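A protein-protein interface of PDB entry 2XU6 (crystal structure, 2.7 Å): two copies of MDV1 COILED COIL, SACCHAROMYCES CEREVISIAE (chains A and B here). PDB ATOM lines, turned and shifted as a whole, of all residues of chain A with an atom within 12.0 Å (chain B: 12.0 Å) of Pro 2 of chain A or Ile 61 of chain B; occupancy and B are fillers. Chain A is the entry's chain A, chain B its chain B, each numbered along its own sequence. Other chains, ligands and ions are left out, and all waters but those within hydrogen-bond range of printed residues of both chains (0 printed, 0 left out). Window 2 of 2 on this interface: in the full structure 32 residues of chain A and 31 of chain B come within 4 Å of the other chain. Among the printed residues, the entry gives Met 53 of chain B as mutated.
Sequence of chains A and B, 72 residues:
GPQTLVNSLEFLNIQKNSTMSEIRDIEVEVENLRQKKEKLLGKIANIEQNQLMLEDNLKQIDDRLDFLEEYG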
ATOM      1  N   GLY A   1     -24.362  16.599  -5.650  1.00  0.00           N
ATOM      2  CA  GLY A   1     -23.397  17.448  -4.891  1.00  0.00           C
ATOM      3  C   GLY A   1     -24.078  18.704  -4.374  1.00  0.00           C
ATOM      4  O   GLY A   1     -25.293  18.810  -4.448  1.00  0.00           O
ATOM      5  N   PRO A   2     -23.298  19.675  -3.870  1.00  0.00           N
ATOM      6  CA  PRO A   2     -23.882  20.858  -3.210  1.00  0.00           C
ATOM      7  C   PRO A   2     -24.794  21.691  -4.133  1.00  0.00           C
ATOM      8  O   PRO A   2     -25.712  22.360  -3.655  1.00  0.00           O
ATOM      9  CB  PRO A   2     -22.648  21.683  -2.802  1.00  0.00           C
ATOM     10  CG  PRO A   2     -21.621  21.340  -3.877  1.00  0.00           C
ATOM     11  CD  PRO A   2     -21.854  19.849  -4.143  1.00  0.00           C
ATOM     12  N   GLN A   3     -24.538  21.665  -5.436  1.00  0.00           N
ATOM     13  CA  GLN A   3     -25.389  22.396  -6.342  1.00  0.00           C
ATOM     14  C   GLN A   3     -26.726  21.689  -6.394  1.00  0.00           C
ATOM     15  O   GLN A   3     -27.749  22.287  -6.089  1.00  0.00           O
ATOM     16  CB  GLN A   3     -24.781  22.521  -7.728  1.00  0.00           C
ATOM     17  CG  GLN A   3     -25.490  23.535  -8.567  1.00  0.00           C
ATOM     18  CD  GLN A   3     -25.578  24.885  -7.880  1.00  0.00           C
ATOM     19  OE1 GLN A   3     -24.571  25.514  -7.607  1.00  0.00           O
ATOM     20  NE2 GLN A   3     -26.793  25.331  -7.596  1.00  0.00           N
ATOM     21  N   THR A   4     -26.704  20.411  -6.750  1.00  0.00           N
ATOM     22  CA  THR A   4     -27.894  19.584  -6.759  1.00  0.00           C
ATOM     23  C   THR A   4     -28.732  19.776  -5.503  1.00  0.00           C
ATOM     24  O   THR A   4     -29.943  19.886  -5.576  1.00  0.00           O
ATOM     25  CB  THR A   4     -27.520  18.117  -6.912  1.00  0.00           C
ATOM     26  OG1 THR A   4     -27.614  17.777  -8.293  1.00  0.00           O
ATOM     27  CG2 THR A   4     -28.462  17.209  -6.116  1.00  0.00           C
ATOM     28  N   LEU A   5     -28.072  19.834  -4.358  1.00  0.00           N
ATOM     29  CA  LEU A   5     -28.725  20.012  -3.076  1.00  0.00           C
ATOM     30  C   LEU A   5     -29.272  21.418  -2.932  1.00  0.00           C
ATOM     31  O   LEU A   5     -30.281  21.624  -2.302  1.00  0.00           O
ATOM     32  CB  LEU A   5     -27.739  19.739  -1.949  1.00  0.00           C
ATOM     33  CG  LEU A   5     -28.403  19.170  -0.707  1.00  0.00           C
ATOM     34  CD1 LEU A   5     -27.534  18.091  -0.115  1.00  0.00           C
ATOM     35  CD2 LEU A   5     -28.697  20.251   0.292  1.00  0.00           C
ATOM     36  N   VAL A   6     -28.586  22.398  -3.498  1.00  0.00           N
ATOM     37  CA  VAL A   6     -29.070  23.765  -3.366  1.00  0.00           C
ATOM     38  C   VAL A   6     -30.283  23.989  -4.287  1.00  0.00           C
ATOM     39  O   VAL A   6     -31.305  24.515  -3.851  1.00  0.00           O
ATOM     40  CB  VAL A   6     -27.935  24.805  -3.520  1.00  0.00           C
ATOM     41  CG1 VAL A   6     -28.472  26.154  -3.943  1.00  0.00           C
ATOM     42  CG2 VAL A   6     -27.190  24.932  -2.196  1.00  0.00           C
ATOM     43  N   ASN A   7     -30.156  23.562  -5.542  1.00  0.00           N
ATOM     44  CA  ASN A   7     -31.256  23.509  -6.486  1.00  0.00           C
ATOM     45  C   ASN A   7     -32.499  22.809  -5.955  1.00  0.00           C
ATOM     46  O   ASN A   7     -33.625  23.182  -6.283  1.00  0.00           O
ATOM     47  CB  ASN A   7     -30.812  22.766  -7.738  1.00  0.00           C
ATOM     48  CG  ASN A   7     -29.742  23.501  -8.496  1.00  0.00           C
ATOM     49  OD1 ASN A   7     -29.410  24.637  -8.170  1.00  0.00           O
ATOM     50  ND2 ASN A   7     -29.190  22.854  -9.514  1.00  0.00           N
ATOM     51  N   SER A   8     -32.290  21.765  -5.167  1.00  0.00           N
ATOM     52  CA  SER A   8     -33.390  20.986  -4.660  1.00  0.00           C
ATOM     53  C   SER A   8     -34.074  21.703  -3.527  1.00  0.00           C
ATOM     54  O   SER A   8     -35.288  21.819  -3.539  1.00  0.00           O
ATOM     55  CB  SER A   8     -32.951  19.594  -4.257  1.00  0.00           C
ATOM     56  OG  SER A   8     -33.131  18.741  -5.368  1.00  0.00           O
ATOM     57  N   LEU A   9     -33.309  22.201  -2.561  1.00  0.00           N
ATOM     58  CA  LEU A   9     -33.889  22.951  -1.464  1.00  0.00           C
ATOM     59  C   LEU A   9     -34.706  24.139  -1.993  1.00  0.00           C
ATOM     60  O   LEU A   9     -35.835  24.367  -1.562  1.00  0.00           O
ATOM     61  CB  LEU A   9     -32.813  23.402  -0.476  1.00  0.00           C
ATOM     62  CG  LEU A   9     -32.154  22.309   0.382  1.00  0.00           C
ATOM     63  CD1 LEU A   9     -30.799  22.748   0.924  1.00  0.00           C
ATOM     64  CD2 LEU A   9     -33.043  21.865   1.528  1.00  0.00           C
ATOM     65  N   GLU A  10     -34.157  24.868  -2.955  1.00  0.00           N
ATOM     66  CA  GLU A  10     -34.819  26.027  -3.515  1.00  0.00           C
ATOM     67  C   GLU A  10     -36.151  25.670  -4.157  1.00  0.00           C
ATOM     68  O   GLU A  10     -37.137  26.351  -3.941  1.00  0.00           O
ATOM     69  CB  GLU A  10     -33.902  26.676  -4.535  1.00  0.00           C
ATOM     70  CG  GLU A  10     -34.508  27.853  -5.256  1.00  0.00           C
ATOM     71  CD  GLU A  10     -33.657  28.272  -6.439  1.00  0.00           C
ATOM     72  OE1 GLU A  10     -32.396  28.275  -6.286  1.00  0.00           O
ATOM     73  OE2 GLU A  10     -34.251  28.581  -7.516  1.00  0.00           O
ATOM     74  N   PHE A  11     -36.170  24.603  -4.940  1.00  0.00           N
ATOM     75  CA  PHE A  11     -37.374  24.146  -5.592  1.00  0.00           C
ATOM     76  C   PHE A  11     -38.430  23.875  -4.547  1.00  0.00           C
ATOM     77  O   PHE A  11     -39.486  24.474  -4.578  1.00  0.00           O
ATOM     78  CB  PHE A  11     -37.062  22.890  -6.374  1.00  0.00           C
ATOM     79  CG  PHE A  11     -38.249  22.237  -7.021  1.00  0.00           C
ATOM     80  CD1 PHE A  11     -38.626  22.578  -8.309  1.00  0.00           C
ATOM     81  CD2 PHE A  11     -38.943  21.218  -6.370  1.00  0.00           C
ATOM     82  CE1 PHE A  11     -39.700  21.942  -8.942  1.00  0.00           C
ATOM     83  CE2 PHE A  11     -40.013  20.572  -6.988  1.00  0.00           C
ATOM     84  CZ  PHE A  11     -40.391  20.934  -8.281  1.00  0.00           C
ATOM     85  N   GLN B  51     -36.948  18.889   3.163  1.00  0.00           N
ATOM     86  CA  GLN B  51     -35.878  19.876   3.213  1.00  0.00           C
ATOM     87  C   GLN B  51     -34.811  19.616   4.276  1.00  0.00           C
ATOM     88  O   GLN B  51     -33.644  19.912   4.060  1.00  0.00           O
ATOM     89  CB  GLN B  51     -36.446  21.267   3.451  1.00  0.00           C
ATOM     90  CG  GLN B  51     -37.166  21.820   2.277  1.00  0.00           C
ATOM     91  CD  GLN B  51     -37.585  23.261   2.465  1.00  0.00           C
ATOM     92  OE1 GLN B  51     -38.074  23.671   3.528  1.00  0.00           O
ATOM     93  NE2 GLN B  51     -37.419  24.043   1.408  1.00  0.00           N
ATOM     94  N   LEU B  52     -35.184  19.092   5.432  1.00  0.00           N
ATOM     95  CA  LEU B  52     -34.185  18.970   6.476  1.00  0.00           C
ATOM     96  C   LEU B  52     -33.377  17.677   6.323  1.00  0.00           C
ATOM     97  O   LEU B  52     -32.284  17.557   6.850  1.00  0.00           O
ATOM     98  CB  LEU B  52     -34.797  19.121   7.872  1.00  0.00           C
ATOM     99  CG  LEU B  52     -33.787  19.727   8.866  1.00  0.00           C
ATOM    100  CD1 LEU B  52     -34.223  21.110   9.428  1.00  0.00           C
ATOM    101  CD2 LEU B  52     -33.409  18.737  10.003  1.00  0.00           C
ATOM    102  N   MET B  53     -33.920  16.715   5.591  1.00  0.00           N
ATOM    103  CA  MET B  53     -33.187  15.508   5.251  1.00  0.00           C
ATOM    104  C   MET B  53     -32.291  15.808   4.061  1.00  0.00           C
ATOM    105  O   MET B  53     -31.555  14.959   3.592  1.00  0.00           O
ATOM    106  CB  MET B  53     -34.148  14.373   4.917  1.00  0.00           C
ATOM    107  CG  MET B  53     -35.089  13.983   6.038  1.00  0.00           C
ATOM    108  SD  MET B  53     -35.785  12.162   5.826  1.00  0.00           S
ATOM    109  CE  MET B  53     -34.435  11.139   6.788  1.00  0.00           C
ATOM    110  N   LEU B  54     -32.382  17.030   3.568  1.00  0.00           N
ATOM    111  CA  LEU B  54     -31.461  17.510   2.580  1.00  0.00           C
ATOM    112  C   LEU B  54     -30.415  18.351   3.293  1.00  0.00           C
ATOM    113  O   LEU B  54     -29.282  17.914   3.344  1.00  0.00           O
ATOM    114  CB  LEU B  54     -32.174  18.277   1.468  1.00  0.00           C
ATOM    115  CG  LEU B  54     -33.189  17.490   0.629  1.00  0.00           C
ATOM    116  CD1 LEU B  54     -33.643  18.318  -0.562  1.00  0.00           C
ATOM    117  CD2 LEU B  54     -32.649  16.142   0.175  1.00  0.00           C
ATOM    118  N   GLU B  55     -30.793  19.509   3.868  1.00  0.00           N
ATOM    119  CA  GLU B  55     -29.886  20.385   4.651  1.00  0.00           C
ATOM    120  C   GLU B  55     -28.903  19.595   5.514  1.00  0.00           C
ATOM    121  O   GLU B  55     -27.824  20.090   5.848  1.00  0.00           O
ATOM    122  CB  GLU B  55     -30.689  21.338   5.546  1.00  0.00           C
ATOM    123  CG  GLU B  55     -29.851  22.396   6.251  1.00  0.00           C
ATOM    124  CD  GLU B  55     -30.414  22.809   7.610  1.00  0.00           C
ATOM    125  OE1 GLU B  55     -31.588  22.492   7.902  1.00  0.00           O
ATOM    126  OE2 GLU B  55     -29.677  23.457   8.388  1.00  0.00           O
ATOM    127  N   ASP B  56     -29.321  18.376   5.892  1.00  0.00           N
ATOM    128  CA  ASP B  56     -28.476  17.392   6.577  1.00  0.00           C
ATOM    129  C   ASP B  56     -27.293  17.035   5.692  1.00  0.00           C
ATOM    130  O   ASP B  56     -26.136  17.274   6.051  1.00  0.00           O
ATOM    131  CB  ASP B  56     -29.283  16.121   6.902  1.00  0.00           C
ATOM    132  CG  ASP B  56     -28.465  14.850   6.751  1.00  0.00           C
ATOM    133  OD1 ASP B  56     -27.663  14.554   7.658  1.00  0.00           O
ATOM    134  OD2 ASP B  56     -28.619  14.158   5.717  1.00  0.00           O
ATOM    135  N   ASN B  57     -27.610  16.453   4.538  1.00  0.00           N
ATOM    136  CA  ASN B  57     -26.640  16.026   3.551  1.00  0.00           C
ATOM    137  C   ASN B  57     -25.664  17.125   3.096  1.00  0.00           C
ATOM    138  O   ASN B  57     -24.474  16.864   2.923  1.00  0.00           O
ATOM    139  CB  ASN B  57     -27.404  15.495   2.356  1.00  0.00           C
ATOM    140  CG  ASN B  57     -26.851  14.215   1.857  1.00  0.00           C
ATOM    141  OD1 ASN B  57     -26.518  14.093   0.672  1.00  0.00           O
ATOM    142  ND2 ASN B  57     -26.750  13.226   2.754  1.00  0.00           N
ATOM    143  N   LEU B  58     -26.187  18.343   2.925  1.00  0.00           N
ATOM    144  CA  LEU B  58     -25.435  19.496   2.447  1.00  0.00           C
ATOM    145  C   LEU B  58     -24.336  19.841   3.408  1.00  0.00           C
ATOM    146  O   LEU B  58     -23.175  19.944   3.014  1.00  0.00           O
ATOM    147  CB  LEU B  58     -26.337  20.729   2.274  1.00  0.00           C
ATOM    148  CG  LEU B  58     -25.707  22.071   1.843  1.00  0.00           C
ATOM    149  CD1 LEU B  58     -25.316  22.092   0.353  1.00  0.00           C
ATOM    150  CD2 LEU B  58     -26.629  23.239   2.166  1.00  0.00           C
ATOM    151  N   LYS B  59     -24.694  20.040   4.668  1.00  0.00           N
ATOM    152  CA  LYS B  59     -23.701  20.470   5.649  1.00  0.00           C
ATOM    153  C   LYS B  59     -22.874  19.300   6.238  1.00  0.00           C
ATOM    154  O   LYS B  59     -21.922  19.524   6.984  1.00  0.00           O
ATOM    155  CB  LYS B  59     -24.327  21.419   6.687  1.00  0.00           C
ATOM    156  CG  LYS B  59     -24.625  22.822   6.098  1.00  0.00           C
ATOM    157  CD  LYS B  59     -26.105  23.232   6.255  1.00  0.00           C
ATOM    158  CE  LYS B  59     -26.393  24.584   5.584  1.00  0.00           C
ATOM    159  NZ  LYS B  59     -27.840  24.962   5.626  1.00  0.00           N
ATOM    160  N   GLN B  60     -23.222  18.066   5.862  1.00  0.00           N
ATOM    161  CA  GLN B  60     -22.337  16.913   6.046  1.00  0.00           C
ATOM    162  C   GLN B  60     -21.279  16.884   4.949  1.00  0.00           C
ATOM    163  O   GLN B  60     -20.113  16.567   5.203  1.00  0.00           O
ATOM    164  CB  GLN B  60     -23.119  15.601   6.065  1.00  0.00           C
ATOM    165  CG  GLN B  60     -23.713  15.271   7.434  1.00  0.00           C
ATOM    166  CD  GLN B  60     -24.443  13.932   7.475  1.00  0.00           C
ATOM    167  OE1 GLN B  60     -25.032  13.492   6.482  1.00  0.00           O
ATOM    168  NE2 GLN B  60     -24.415  13.284   8.636  1.00  0.00           N
ATOM    169  N   ILE B  61     -21.686  17.228   3.729  1.00  0.00           N
ATOM    170  CA  ILE B  61     -20.742  17.324   2.619  1.00  0.00           C
ATOM    171  C   ILE B  61     -19.975  18.636   2.654  1.00  0.00           C
ATOM    172  O   ILE B  61     -18.975  18.772   1.963  1.00  0.00           O
ATOM    173  CB  ILE B  61     -21.406  17.118   1.213  1.00  0.00           C
ATOM    174  CG1 ILE B  61     -22.239  18.351   0.800  1.00  0.00           C
ATOM    175  CG2 ILE B  61     -22.163  15.752   1.145  1.00  0.00           C
ATOM    176  CD1 ILE B  61     -22.996  18.233  -0.523  1.00  0.00           C
ATOM    177  N   ASP B  62     -20.423  19.587   3.471  1.00  0.00           N
ATOM    178  CA  ASP B  62     -19.788  20.911   3.521  1.00  0.00           C
ATOM    179  C   ASP B  62     -18.474  20.917   4.322  1.00  0.00           C
ATOM    180  O   ASP B  62     -17.932  21.985   4.661  1.00  0.00           O
ATOM    181  CB  ASP B  62     -20.763  21.983   4.025  1.00  0.00           C
ATOM    182  CG  ASP B  62     -20.747  23.243   3.158  1.00  0.00           C
ATOM    183  OD1 ASP B  62     -20.954  23.141   1.923  1.00  0.00           O
ATOM    184  OD2 ASP B  62     -20.531  24.340   3.717  1.00  0.00           O
ATOM    185  N   ASP B  63     -17.986  19.706   4.606  1.00  0.00           N
ATOM    186  CA  ASP B  63     -16.656  19.438   5.187  1.00  0.00           C
ATOM    187  C   ASP B  63     -16.165  18.022   4.800  1.00  0.00           C
ATOM    188  O   ASP B  63     -15.142  17.546   5.310  1.00  0.00           O
ATOM    189  CB  ASP B  63     -16.674  19.622   6.711  1.00  0.00           C
ATOM    190  CG  ASP B  63     -17.895  18.993   7.363  1.00  0.00           C
ATOM    191  OD1 ASP B  63     -18.603  19.711   8.100  1.00  0.00           O
ATOM    192  OD2 ASP B  63     -18.155  17.789   7.131  1.00  0.00           O
ATOM    193  N   ARG B  64     -16.924  17.368   3.908  1.00  0.00           N
ATOM    194  CA  ARG B  64     -16.553  16.109   3.235  1.00  0.00           C
ATOM    195  C   ARG B  64     -15.652  15.193   4.072  1.00  0.00           C
ATOM    196  O   ARG B  64     -15.075  14.230   3.568  1.00  0.00           O
ATOM    197  CB  ARG B  64     -15.932  16.407   1.856  1.00  0.00           C
ATOM    198  CG  ARG B  64     -14.538  17.047   1.898  1.00  0.00           C
ATOM    199  CD  ARG B  64     -14.463  18.335   1.074  1.00  0.00           C
ATOM    200  NE  ARG B  64     -15.034  19.484   1.782  1.00  0.00           N
ATOM    201  CZ  ARG B  64     -15.071  20.732   1.312  1.00  0.00           C
ATOM    202  NH1 ARG B  64     -14.569  21.024   0.114  1.00  0.00           N
ATOM    203  NH2 ARG B  64     -15.616  21.697   2.049  1.00  0.00           N
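No position is printed for both chains. Of the 7 pairs that touch across the chains among the printed residues, none has its exchanged pair printed and touching as well.
The backbone carbonyl oxygen (O) of Leu 9 of chain A sits at hydrogen-bond distance from the side-chain amide nitrogen (NE2) of Gln 51 of chain B (3.4 Å).
Pro 2 of chain A touches just one residue of chain B: Ile 61. No residue of chain B comes within 4 Å of Gln 3 of chain A. No residue of chain B comes within 4 Å of Thr 4 of chain A. Asn 7 of chain A touches none of the printed residues of chain B. Printed residues of chain B within 4 Å of Ser 8 of chain A: Leu 54. Printed residues of chain B within 4 Å of Leu 9 of chain A: Gln 51 (3.3 Å) and Leu 54 (3.7 Å). Met 53 of chain B touches none of the printed residues of chain A. Of the printed residues of chain A, Asn 57 of chain B touches Leu 5. Of the printed residues of chain A, Leu 58 of chain B touches Leu 5 (3.1 Å). Printed residues of chain A within 4 Å of Ile 61 of chain B: Pro 2. No residue of chain A comes within 4 Å of Arg 64 of chain B.
Of the 14 printed residues of chain B, 5 touch a printed residue of chain A. Hydrophobic or aromatic side chains of chain B within 4 Å of the printed part of chain A: Leu 54, Leu 58 and Ile 61. Of the 11 printed residues of chain A, 4 touch a printed residue of chain B. Among the printed residues, 7 pairs touch across the chains. Among the printed residues, no Asp or Glu carboxylate lies within 4 Å of a Lys or Arg side-chain nitrogen of the other chain.
The side-chain hydroxyl (OG) of Ser 8 of chain A sits close to the backbone carbonyl oxygen (O) of Thr 4 of chain A (3.4 Å).
Among the printed residues, pairs that only touch across the chains: Pro 2 of chain A with Ile 61 of chain B (3.7 Å), Leu 5 of chain A with Leu 54 of chain B (3.9 Å), Leu 5 of chain A with Asn 57 of chain B (3.6 Å), Leu 5 of chain A with Leu 58 of chain B (3.1 Å), Ser 8 of chain A with Leu 54 of chain B (3.97 Å) and Leu 9 of chain A with Leu 54 of chain B (3.7 Å).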
